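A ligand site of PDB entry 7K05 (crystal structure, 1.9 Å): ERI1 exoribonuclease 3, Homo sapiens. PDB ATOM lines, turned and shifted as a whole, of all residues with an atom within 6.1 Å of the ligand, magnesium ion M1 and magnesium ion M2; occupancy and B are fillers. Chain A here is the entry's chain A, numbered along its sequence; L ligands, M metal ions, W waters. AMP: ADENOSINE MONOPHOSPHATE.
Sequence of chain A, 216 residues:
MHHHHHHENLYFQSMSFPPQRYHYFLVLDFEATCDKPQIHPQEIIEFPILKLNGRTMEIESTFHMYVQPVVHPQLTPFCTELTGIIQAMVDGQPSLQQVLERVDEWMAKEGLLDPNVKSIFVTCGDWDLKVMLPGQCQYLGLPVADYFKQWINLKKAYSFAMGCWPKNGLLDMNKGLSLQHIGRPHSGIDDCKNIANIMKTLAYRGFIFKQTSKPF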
ATOM      1  N   LEU A  28     -18.271 -21.842 -36.287  1.00  0.00           N
ATOM      2  CA  LEU A  28     -17.326 -22.665 -35.554  1.00  0.00           C
ATOM      3  C   LEU A  28     -17.340 -22.308 -34.070  1.00  0.00           C
ATOM      4  O   LEU A  28     -17.463 -21.123 -33.724  1.00  0.00           O
ATOM      5  CB  LEU A  28     -15.939 -22.490 -36.167  1.00  0.00           C
ATOM      6  CG  LEU A  28     -14.818 -23.276 -35.513  1.00  0.00           C
ATOM      7  CD1 LEU A  28     -13.762 -23.632 -36.511  1.00  0.00           C
ATOM      8  CD2 LEU A  28     -14.183 -22.322 -34.485  1.00  0.00           C
ATOM      9  N   ASP A  29     -17.249 -23.300 -33.178  1.00  0.00           N
ATOM     10  CA  ASP A  29     -17.146 -22.981 -31.755  1.00  0.00           C
ATOM     11  C   ASP A  29     -16.443 -24.116 -31.025  1.00  0.00           C
ATOM     12  O   ASP A  29     -17.069 -25.142 -30.752  1.00  0.00           O
ATOM     13  CB  ASP A  29     -18.529 -22.731 -31.148  1.00  0.00           C
ATOM     14  CG  ASP A  29     -18.406 -22.333 -29.627  1.00  0.00           C
ATOM     15  OD1 ASP A  29     -18.316 -21.149 -29.367  1.00  0.00           O
ATOM     16  OD2 ASP A  29     -18.391 -23.188 -28.715  1.00  0.00           O
ATOM     17  N   PHE A  30     -15.161 -23.944 -30.729  1.00  0.00           N
ATOM     18  CA  PHE A  30     -14.407 -25.038 -30.135  1.00  0.00           C
ATOM     19  C   PHE A  30     -14.865 -25.312 -28.730  1.00  0.00           C
ATOM     20  O   PHE A  30     -15.265 -24.372 -28.018  1.00  0.00           O
ATOM     21  CB  PHE A  30     -12.906 -24.695 -30.032  1.00  0.00           C
ATOM     22  CG  PHE A  30     -12.215 -24.492 -31.353  1.00  0.00           C
ATOM     23  CD1 PHE A  30     -12.310 -25.473 -32.361  1.00  0.00           C
ATOM     24  CD2 PHE A  30     -11.442 -23.343 -31.584  1.00  0.00           C
ATOM     25  CE1 PHE A  30     -11.671 -25.332 -33.572  1.00  0.00           C
ATOM     26  CE2 PHE A  30     -10.810 -23.153 -32.825  1.00  0.00           C
ATOM     27  CZ  PHE A  30     -10.865 -24.180 -33.810  1.00  0.00           C
ATOM     28  N   GLU A  31     -14.653 -26.551 -28.263  1.00  0.00           N
ATOM     29  CA  GLU A  31     -14.450 -26.754 -26.836  1.00  0.00           C
ATOM     30  C   GLU A  31     -12.996 -27.172 -26.619  1.00  0.00           C
ATOM     31  O   GLU A  31     -12.373 -27.759 -27.493  1.00  0.00           O
ATOM     32  CB  GLU A  31     -15.379 -27.815 -26.246  1.00  0.00           C
ATOM     33  CG  GLU A  31     -16.863 -27.467 -26.415  1.00  0.00           C
ATOM     34  CD  GLU A  31     -17.259 -26.060 -25.908  1.00  0.00           C
ATOM     35  OE1 GLU A  31     -16.787 -25.634 -24.821  1.00  0.00           O
ATOM     36  OE2 GLU A  31     -18.094 -25.421 -26.592  1.00  0.00           O
ATOM     37  N   ALA A  32     -12.458 -26.861 -25.444  1.00  0.00           N
ATOM     38  CA  ALA A  32     -11.068 -27.189 -25.142  1.00  0.00           C
ATOM     39  C   ALA A  32     -10.956 -27.778 -23.750  1.00  0.00           C
ATOM     40  O   ALA A  32     -11.815 -27.537 -22.888  1.00  0.00           O
ATOM     41  CB  ALA A  32     -10.183 -25.909 -25.222  1.00  0.00           C
ATOM     42  N   THR A  33      -9.857 -28.500 -23.507  1.00  0.00           N
ATOM     43  CA  THR A  33      -9.521 -28.907 -22.135  1.00  0.00           C
ATOM     44  C   THR A  33      -9.502 -27.658 -21.227  1.00  0.00           C
ATOM     45  O   THR A  33      -9.221 -26.545 -21.668  1.00  0.00           O
ATOM     46  CB  THR A  33      -8.163 -29.597 -22.060  1.00  0.00           C
ATOM     47  OG1 THR A  33      -7.197 -28.705 -22.634  1.00  0.00           O
ATOM     48  CG2 THR A  33      -8.177 -30.946 -22.899  1.00  0.00           C
ATOM     49  N   CYS A  34      -9.883 -27.837 -19.981  1.00  0.00           N
ATOM     50  CA  CYS A  34      -9.929 -26.714 -19.051  1.00  0.00           C
ATOM     51  C   CYS A  34      -9.868 -27.293 -17.658  1.00  0.00           C
ATOM     52  O   CYS A  34      -9.923 -28.510 -17.486  1.00  0.00           O
ATOM     53  CB  CYS A  34     -11.199 -25.873 -19.201  1.00  0.00           C
ATOM     54  SG  CYS A  34     -12.704 -26.840 -19.326  1.00  0.00           S
ATOM     55  N   ASP A  35      -9.787 -26.377 -16.657  1.00  0.00           N
ATOM     56  CA  ASP A  35      -9.748 -26.756 -15.260  1.00  0.00           C
ATOM     57  C   ASP A  35      -9.968 -25.481 -14.441  1.00  0.00           C
ATOM     58  O   ASP A  35     -10.031 -24.364 -14.981  1.00  0.00           O
ATOM     59  CB  ASP A  35      -8.420 -27.450 -14.907  1.00  0.00           C
ATOM     60  CG  ASP A  35      -8.541 -28.394 -13.651  1.00  0.00           C
ATOM     61  OD1 ASP A  35      -9.643 -28.495 -13.035  1.00  0.00           O
ATOM     62  OD2 ASP A  35      -7.531 -29.072 -13.317  1.00  0.00           O
ATOM     63  N   LYS A  36     -10.060 -25.660 -13.120  1.00  0.00           N
ATOM     64  CA  LYS A  36     -10.101 -24.532 -12.164  1.00  0.00           C
ATOM     65  C   LYS A  36      -8.894 -24.645 -11.250  1.00  0.00           C
ATOM     66  O   LYS A  36      -8.796 -25.649 -10.518  1.00  0.00           O
ATOM     67  CB  LYS A  36     -11.382 -24.556 -11.329  1.00  0.00           C
ATOM     68  CG  LYS A  36     -12.208 -23.263 -11.323  1.00  0.00           C
ATOM     69  CD  LYS A  36     -12.766 -22.987 -12.714  1.00  0.00           C
ATOM     70  CE  LYS A  36     -13.423 -21.641 -12.788  1.00  0.00           C
ATOM     71  NZ  LYS A  36     -13.445 -21.112 -14.151  1.00  0.00           N
ATOM     72  N   GLN A  38      -7.189 -22.390 -14.580  1.00  0.00           N
ATOM     73  CA  GLN A  38      -7.199 -22.887 -15.952  1.00  0.00           C
ATOM     74  C   GLN A  38      -6.005 -23.804 -16.235  1.00  0.00           C
ATOM     75  O   GLN A  38      -4.892 -23.575 -15.754  1.00  0.00           O
ATOM     76  CB  GLN A  38      -7.184 -21.700 -16.903  1.00  0.00           C
ATOM     77  CG  GLN A  38      -7.437 -22.093 -18.362  1.00  0.00           C
ATOM     78  CD  GLN A  38      -8.731 -22.832 -18.491  1.00  0.00           C
ATOM     79  OE1 GLN A  38      -8.770 -24.047 -18.199  1.00  0.00           O
ATOM     80  NE2 GLN A  38      -9.835 -22.128 -18.877  1.00  0.00           N
ATOM     81  N   GLN A  42      -4.145 -25.229 -22.981  1.00  0.00           N
ATOM     82  CA  GLN A  42      -5.448 -25.796 -23.323  1.00  0.00           C
ATOM     83  C   GLN A  42      -5.332 -26.453 -24.676  1.00  0.00           C
ATOM     84  O   GLN A  42      -4.476 -26.074 -25.484  1.00  0.00           O
ATOM     85  CB  GLN A  42      -6.539 -24.728 -23.398  1.00  0.00           C
ATOM     86  CG  GLN A  42      -6.870 -24.015 -22.041  1.00  0.00           C
ATOM     87  CD  GLN A  42      -8.065 -23.068 -22.248  1.00  0.00           C
ATOM     88  OE1 GLN A  42      -7.898 -21.892 -22.589  1.00  0.00           O
ATOM     89  NE2 GLN A  42      -9.272 -23.614 -22.167  1.00  0.00           N
ATOM     90  N   ILE A  45     -10.732 -30.044 -27.934  1.00  0.00           N
ATOM     91  CA  ILE A  45     -11.308 -31.393 -27.845  1.00  0.00           C
ATOM     92  C   ILE A  45     -12.590 -31.552 -28.663  1.00  0.00           C
ATOM     93  O   ILE A  45     -13.106 -32.674 -28.746  1.00  0.00           O
ATOM     94  CB  ILE A  45     -11.555 -31.820 -26.373  1.00  0.00           C
ATOM     95  CG1 ILE A  45     -12.510 -30.803 -25.688  1.00  0.00           C
ATOM     96  CG2 ILE A  45     -10.237 -31.964 -25.586  1.00  0.00           C
ATOM     97  CD1 ILE A  45     -12.836 -31.181 -24.217  1.00  0.00           C
ATOM     98  N   PHE A  78     -13.873 -30.895 -13.994  1.00  0.00           N
ATOM     99  CA  PHE A  78     -14.399 -29.602 -14.385  1.00  0.00           C
ATOM    100  C   PHE A  78     -14.726 -29.567 -15.880  1.00  0.00           C
ATOM    101  O   PHE A  78     -15.807 -29.119 -16.281  1.00  0.00           O
ATOM    102  CB  PHE A  78     -13.414 -28.493 -14.043  1.00  0.00           C
ATOM    103  CG  PHE A  78     -13.917 -27.147 -14.493  1.00  0.00           C
ATOM    104  CD1 PHE A  78     -14.873 -26.486 -13.734  1.00  0.00           C
ATOM    105  CD2 PHE A  78     -13.530 -26.614 -15.697  1.00  0.00           C
ATOM    106  CE1 PHE A  78     -15.378 -25.311 -14.137  1.00  0.00           C
ATOM    107  CE2 PHE A  78     -14.038 -25.423 -16.161  1.00  0.00           C
ATOM    108  CZ  PHE A  78     -15.002 -24.767 -15.370  1.00  0.00           C
ATOM    109  N   LEU A  82     -18.251 -28.905 -17.412  1.00  0.00           N
ATOM    110  CA  LEU A  82     -18.544 -27.729 -18.232  1.00  0.00           C
ATOM    111  C   LEU A  82     -19.134 -28.115 -19.588  1.00  0.00           C
ATOM    112  O   LEU A  82     -20.219 -27.625 -19.974  1.00  0.00           O
ATOM    113  CB  LEU A  82     -17.276 -26.907 -18.443  1.00  0.00           C
ATOM    114  CG  LEU A  82     -17.553 -25.601 -19.180  1.00  0.00           C
ATOM    115  CD1 LEU A  82     -18.256 -24.631 -18.171  1.00  0.00           C
ATOM    116  CD2 LEU A  82     -16.200 -25.070 -19.648  1.00  0.00           C
ATOM    117  N   THR A  83     -18.467 -29.027 -20.293  1.00  0.00           N
ATOM    118  CA  THR A  83     -18.725 -29.272 -21.721  1.00  0.00           C
ATOM    119  C   THR A  83     -19.621 -30.455 -21.994  1.00  0.00           C
ATOM    120  O   THR A  83     -20.165 -30.540 -23.101  1.00  0.00           O
ATOM    121  CB  THR A  83     -17.443 -29.561 -22.490  1.00  0.00           C
ATOM    122  OG1 THR A  83     -16.880 -30.783 -22.017  1.00  0.00           O
ATOM    123  CG2 THR A  83     -16.397 -28.361 -22.346  1.00  0.00           C
ATOM    124  N   CYS A 124     -18.323 -16.908 -31.894  1.00  0.00           N
ATOM    125  CA  CYS A 124     -18.821 -16.050 -30.817  1.00  0.00           C
ATOM    126  C   CYS A 124     -17.589 -15.576 -30.032  1.00  0.00           C
ATOM    127  O   CYS A 124     -17.052 -16.344 -29.220  1.00  0.00           O
ATOM    128  CB  CYS A 124     -19.785 -16.816 -29.930  1.00  0.00           C
ATOM    129  SG  CYS A 124     -20.443 -15.760 -28.579  1.00  0.00           S
ATOM    130  N   TRP A 127     -11.852 -15.488 -29.556  1.00  0.00           N
ATOM    131  CA  TRP A 127     -10.947 -16.451 -28.913  1.00  0.00           C
ATOM    132  C   TRP A 127     -10.594 -17.619 -29.830  1.00  0.00           C
ATOM    133  O   TRP A 127      -9.440 -18.053 -29.887  1.00  0.00           O
ATOM    134  CB  TRP A 127     -11.598 -16.996 -27.647  1.00  0.00           C
ATOM    135  CG  TRP A 127     -10.754 -17.972 -26.865  1.00  0.00           C
ATOM    136  CD1 TRP A 127      -9.626 -17.695 -26.081  1.00  0.00           C
ATOM    137  CD2 TRP A 127     -10.929 -19.377 -26.832  1.00  0.00           C
ATOM    138  NE1 TRP A 127      -9.125 -18.864 -25.568  1.00  0.00           N
ATOM    139  CE2 TRP A 127      -9.917 -19.907 -26.006  1.00  0.00           C
ATOM    140  CE3 TRP A 127     -11.882 -20.229 -27.390  1.00  0.00           C
ATOM    141  CZ2 TRP A 127      -9.824 -21.251 -25.745  1.00  0.00           C
ATOM    142  CZ3 TRP A 127     -11.765 -21.596 -27.129  1.00  0.00           C
ATOM    143  CH2 TRP A 127     -10.753 -22.070 -26.292  1.00  0.00           C
ATOM    144  N   ASP A 128     -11.587 -18.223 -30.485  1.00  0.00           N
ATOM    145  CA  ASP A 128     -11.339 -19.483 -31.210  1.00  0.00           C
ATOM    146  C   ASP A 128     -10.244 -19.360 -32.260  1.00  0.00           C
ATOM    147  O   ASP A 128      -9.327 -20.186 -32.298  1.00  0.00           O
ATOM    148  CB  ASP A 128     -12.627 -19.939 -31.906  1.00  0.00           C
ATOM    149  CG  ASP A 128     -13.761 -20.113 -30.926  1.00  0.00           C
ATOM    150  OD1 ASP A 128     -14.152 -21.262 -30.648  1.00  0.00           O
ATOM    151  OD2 ASP A 128     -14.253 -19.106 -30.370  1.00  0.00           O
ATOM    152  N   PRO A 185     -25.690 -25.309 -23.313  1.00  0.00           N
ATOM    153  CA  PRO A 185     -24.538 -24.367 -23.355  1.00  0.00           C
ATOM    154  C   PRO A 185     -23.214 -25.118 -23.203  1.00  0.00           C
ATOM    155  O   PRO A 185     -23.128 -26.115 -22.492  1.00  0.00           O
ATOM    156  CB  PRO A 185     -24.771 -23.448 -22.144  1.00  0.00           C
ATOM    157  CG  PRO A 185     -26.307 -23.531 -21.936  1.00  0.00           C
ATOM    158  CD  PRO A 185     -26.681 -24.939 -22.266  1.00  0.00           C
ATOM    159  N   HIS A 186     -22.172 -24.608 -23.853  1.00  0.00           N
ATOM    160  CA  HIS A 186     -20.817 -25.195 -23.833  1.00  0.00           C
ATOM    161  C   HIS A 186     -20.694 -26.564 -24.483  1.00  0.00           C
ATOM    162  O   HIS A 186     -19.662 -27.229 -24.340  1.00  0.00           O
ATOM    163  CB  HIS A 186     -20.262 -25.281 -22.419  1.00  0.00           C
ATOM    164  CG  HIS A 186     -20.393 -23.999 -21.671  1.00  0.00           C
ATOM    165  ND1 HIS A 186     -19.574 -22.924 -21.919  1.00  0.00           N
ATOM    166  CD2 HIS A 186     -21.311 -23.588 -20.756  1.00  0.00           C
ATOM    167  CE1 HIS A 186     -19.938 -21.911 -21.147  1.00  0.00           C
ATOM    168  NE2 HIS A 186     -20.990 -22.294 -20.431  1.00  0.00           N
ATOM    169  N   SER A 187     -21.702 -27.009 -25.194  1.00  0.00           N
ATOM    170  CA  SER A 187     -21.496 -28.040 -26.217  1.00  0.00           C
ATOM    171  C   SER A 187     -21.132 -27.327 -27.523  1.00  0.00           C
ATOM    172  O   SER A 187     -21.844 -26.412 -27.953  1.00  0.00           O
ATOM    173  CB  SER A 187     -22.764 -28.894 -26.403  1.00  0.00           C
ATOM    174  OG  SER A 187     -22.783 -29.494 -27.710  1.00  0.00           O
ATOM    175  N   GLY A 188     -20.031 -27.751 -28.157  1.00  0.00           N
ATOM    176  CA  GLY A 188     -19.554 -27.011 -29.330  1.00  0.00           C
ATOM    177  C   GLY A 188     -20.601 -26.950 -30.428  1.00  0.00           C
ATOM    178  O   GLY A 188     -20.945 -25.884 -30.931  1.00  0.00           O
ATOM    179  N   ASP A 191     -23.557 -24.802 -29.426  1.00  0.00           N
ATOM    180  CA  ASP A 191     -23.225 -23.373 -29.547  1.00  0.00           C
ATOM    181  C   ASP A 191     -23.320 -22.947 -31.015  1.00  0.00           C
ATOM    182  O   ASP A 191     -23.827 -21.865 -31.334  1.00  0.00           O
ATOM    183  CB  ASP A 191     -21.826 -23.130 -28.972  1.00  0.00           C
ATOM    184  CG  ASP A 191     -21.787 -23.189 -27.400  1.00  0.00           C
ATOM    185  OD1 ASP A 191     -22.836 -23.189 -26.741  1.00  0.00           O
ATOM    186  OD2 ASP A 191     -20.675 -23.203 -26.822  1.00  0.00           O
HETATM  187  P   AMP L   1     -17.269 -21.853 -24.761  1.00  0.00           P
HETATM  188  O1P AMP L   1     -17.401 -21.687 -26.276  1.00  0.00           O
HETATM  189  O2P AMP L   1     -17.804 -23.253 -24.393  1.00  0.00           O
HETATM  190  O3P AMP L   1     -17.977 -20.825 -23.952  1.00  0.00           O
HETATM  191  O5' AMP L   1     -15.778 -21.894 -24.248  1.00  0.00           O
HETATM  192  C5' AMP L   1     -14.693 -22.489 -24.943  1.00  0.00           C
HETATM  193  C4' AMP L   1     -13.708 -23.097 -23.943  1.00  0.00           C
HETATM  194  O4' AMP L   1     -13.313 -22.106 -22.960  1.00  0.00           O
HETATM  195  C3' AMP L   1     -14.248 -24.239 -23.107  1.00  0.00           C
HETATM  196  O3' AMP L   1     -14.272 -25.519 -23.810  1.00  0.00           O
HETATM  197  C2' AMP L   1     -13.306 -24.245 -21.903  1.00  0.00           C
HETATM  198  O2' AMP L   1     -12.040 -24.812 -22.280  1.00  0.00           O
HETATM  199  C1' AMP L   1     -13.079 -22.723 -21.705  1.00  0.00           C
HETATM  200  N9  AMP L   1     -14.068 -22.169 -20.743  1.00  0.00           N
HETATM  201  C8  AMP L   1     -15.304 -21.669 -21.078  1.00  0.00           C
HETATM  202  N7  AMP L   1     -15.991 -21.258 -19.953  1.00  0.00           N
HETATM  203  C5  AMP L   1     -15.135 -21.465 -18.929  1.00  0.00           C
HETATM  204  C6  AMP L   1     -15.209 -21.267 -17.455  1.00  0.00           C
HETATM  205  N6  AMP L   1     -16.312 -20.735 -16.884  1.00  0.00           N
HETATM  206  N1  AMP L   1     -14.165 -21.658 -16.764  1.00  0.00           N
HETATM  207  C2  AMP L   1     -13.056 -22.219 -17.293  1.00  0.00           C
HETATM  208  N3  AMP L   1     -12.905 -22.436 -18.618  1.00  0.00           N
HETATM  209  C4  AMP L   1     -13.907 -22.080 -19.458  1.00  0.00           C
HETATM  210 MG    MG M   1     -16.950 -20.534 -27.726  1.00  0.00          MG
HETATM  211 MG    MG M   2     -18.624 -23.483 -27.008  1.00  0.00          MG
HETATM  212  O   HOH W   1     -16.078 -19.583 -26.041  1.00  0.00           O
HETATM  213  O   HOH W   2     -18.801 -19.655 -27.517  1.00  0.00           O
HETATM  214  O   HOH W   3     -15.266 -21.577 -28.172  1.00  0.00           O
HETATM  215  O   HOH W   4     -14.177 -19.407 -23.773  1.00  0.00           O
HETATM  216  O   HOH W   5     -16.285 -19.076 -28.968  1.00  0.00           O
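Residues that only touch magnesium ion M2: Phe 30 (3.6 Å).
Within 4 Å of magnesium ion M2: Asp 29, Phe 30, Glu 31 and Asp 191.
The nearest printed residue that does not touch magnesium ion M2 is His 186 (4.2 Å).
OD2 of Asp 29 binds magnesium ion M2, at 1.7 Å.
Magnesium ion M2 is bound by OE2 of Glu 31 (2.1 Å).
The side-chain carboxylate (OD2) of Asp 191 is bound to magnesium ion M2, at 2.1 Å.
O1P of the ligand is bound to magnesium ion M2.
Slightly farther from magnesium ion M2 lies O2P of the ligand (2.8 Å).
Merely in contact with the ligand: Phe 30, Phe 78, Leu 82, Thr 83 and Trp 127.
Hydrophobic or aromatic side chains that line the ligand: Ala 32, Phe 78, Leu 82, Trp 127 and His 186.
Within 4 Å of the ligand: Asp 29, Phe 30, Glu 31, Ala 32, Thr 33, Cys 34, Lys 36, Gln 38, Gln 42, Phe 78, Leu 82, Thr 83, Trp 127, His 186 and Asp 191.
The nearest printed residue that does not touch the ligand is Asp 35 (4.4 Å).
The backbone NH of Ile 45 lies within hydrogen-bond range of the backbone carbonyl oxygen of Glu 31 (2.8 Å).
OE2 of Glu 31 sits close to N of Gly 188, 3.4 Å away.
OD1 of Asp 191 sits at hydrogen-bond distance from N of His 186, 3.3 Å away.
The backbone NH (N) of Phe 30 sits at hydrogen-bond distance from the side-chain carboxylate (OD1) of Asp 128 (2.9 Å).
The backbone carbonyl oxygen (O) of Ala 32 lies within hydrogen-bond range of the side-chain sulfur (SG) of Cys 34 (3.7 Å).
The backbone NH (N) of Asp 35 sits at hydrogen-bond distance from the side-chain amide oxygen (OE1) of Gln 38 (3.0 Å).
NE2 of Gln 42 lies within hydrogen-bond range of O of Thr 33, at 3.0 Å.
Water W3 bridges OD1 of Asp 128 (2.7 Å) and O of Phe 30 (2.8 Å).
Water W5 bridges OD2 of Asp 128 (2.5 Å) and O of Cys 124 (2.8 Å).
Magnesium ion M1 is bound by an oxygen (O1P) of the ligand (1.9 Å), water W5 (2.0 Å), water W3 (2.0 Å), water W2 (2.1 Å), water W1 (2.1 Å) and the side-chain carboxylate of Asp 29 (2.2 Å).
Magnesium ion M1 has six donor atoms within binding distance.
Of the 23 residues printed, 1 comes within 4 Å of magnesium ion M1.
The nearest printed residue that does not touch magnesium ion M1 is Asp 128 (4.04 Å).
O3' of the ligand sits at hydrogen-bond distance from N of Ala 32 (2.8 Å).
O2P of the ligand sits at hydrogen-bond distance from ND1 of His 186, 3.1 Å away.
O2' of the ligand lies within hydrogen-bond range of O of Thr 33, 3.4 Å away.
An oxygen (O2') of the ligand lies close to the side-chain sulfur (SG) of Cys 34 (3.6 Å).
N1 of the ligand is in hydrogen-bond range of NZ of Lys 36, 2.8 Å away.
NE2 of Gln 42 is in hydrogen-bond range of O2' of the ligand (3.0 Å).
O2' of the ligand sits at hydrogen-bond distance from O of Ala 32 (2.8 Å).
A nitrogen (N3) of the ligand sits at hydrogen-bond distance from the side-chain amide nitrogen (NE2) of Gln 38 (3.1 Å).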
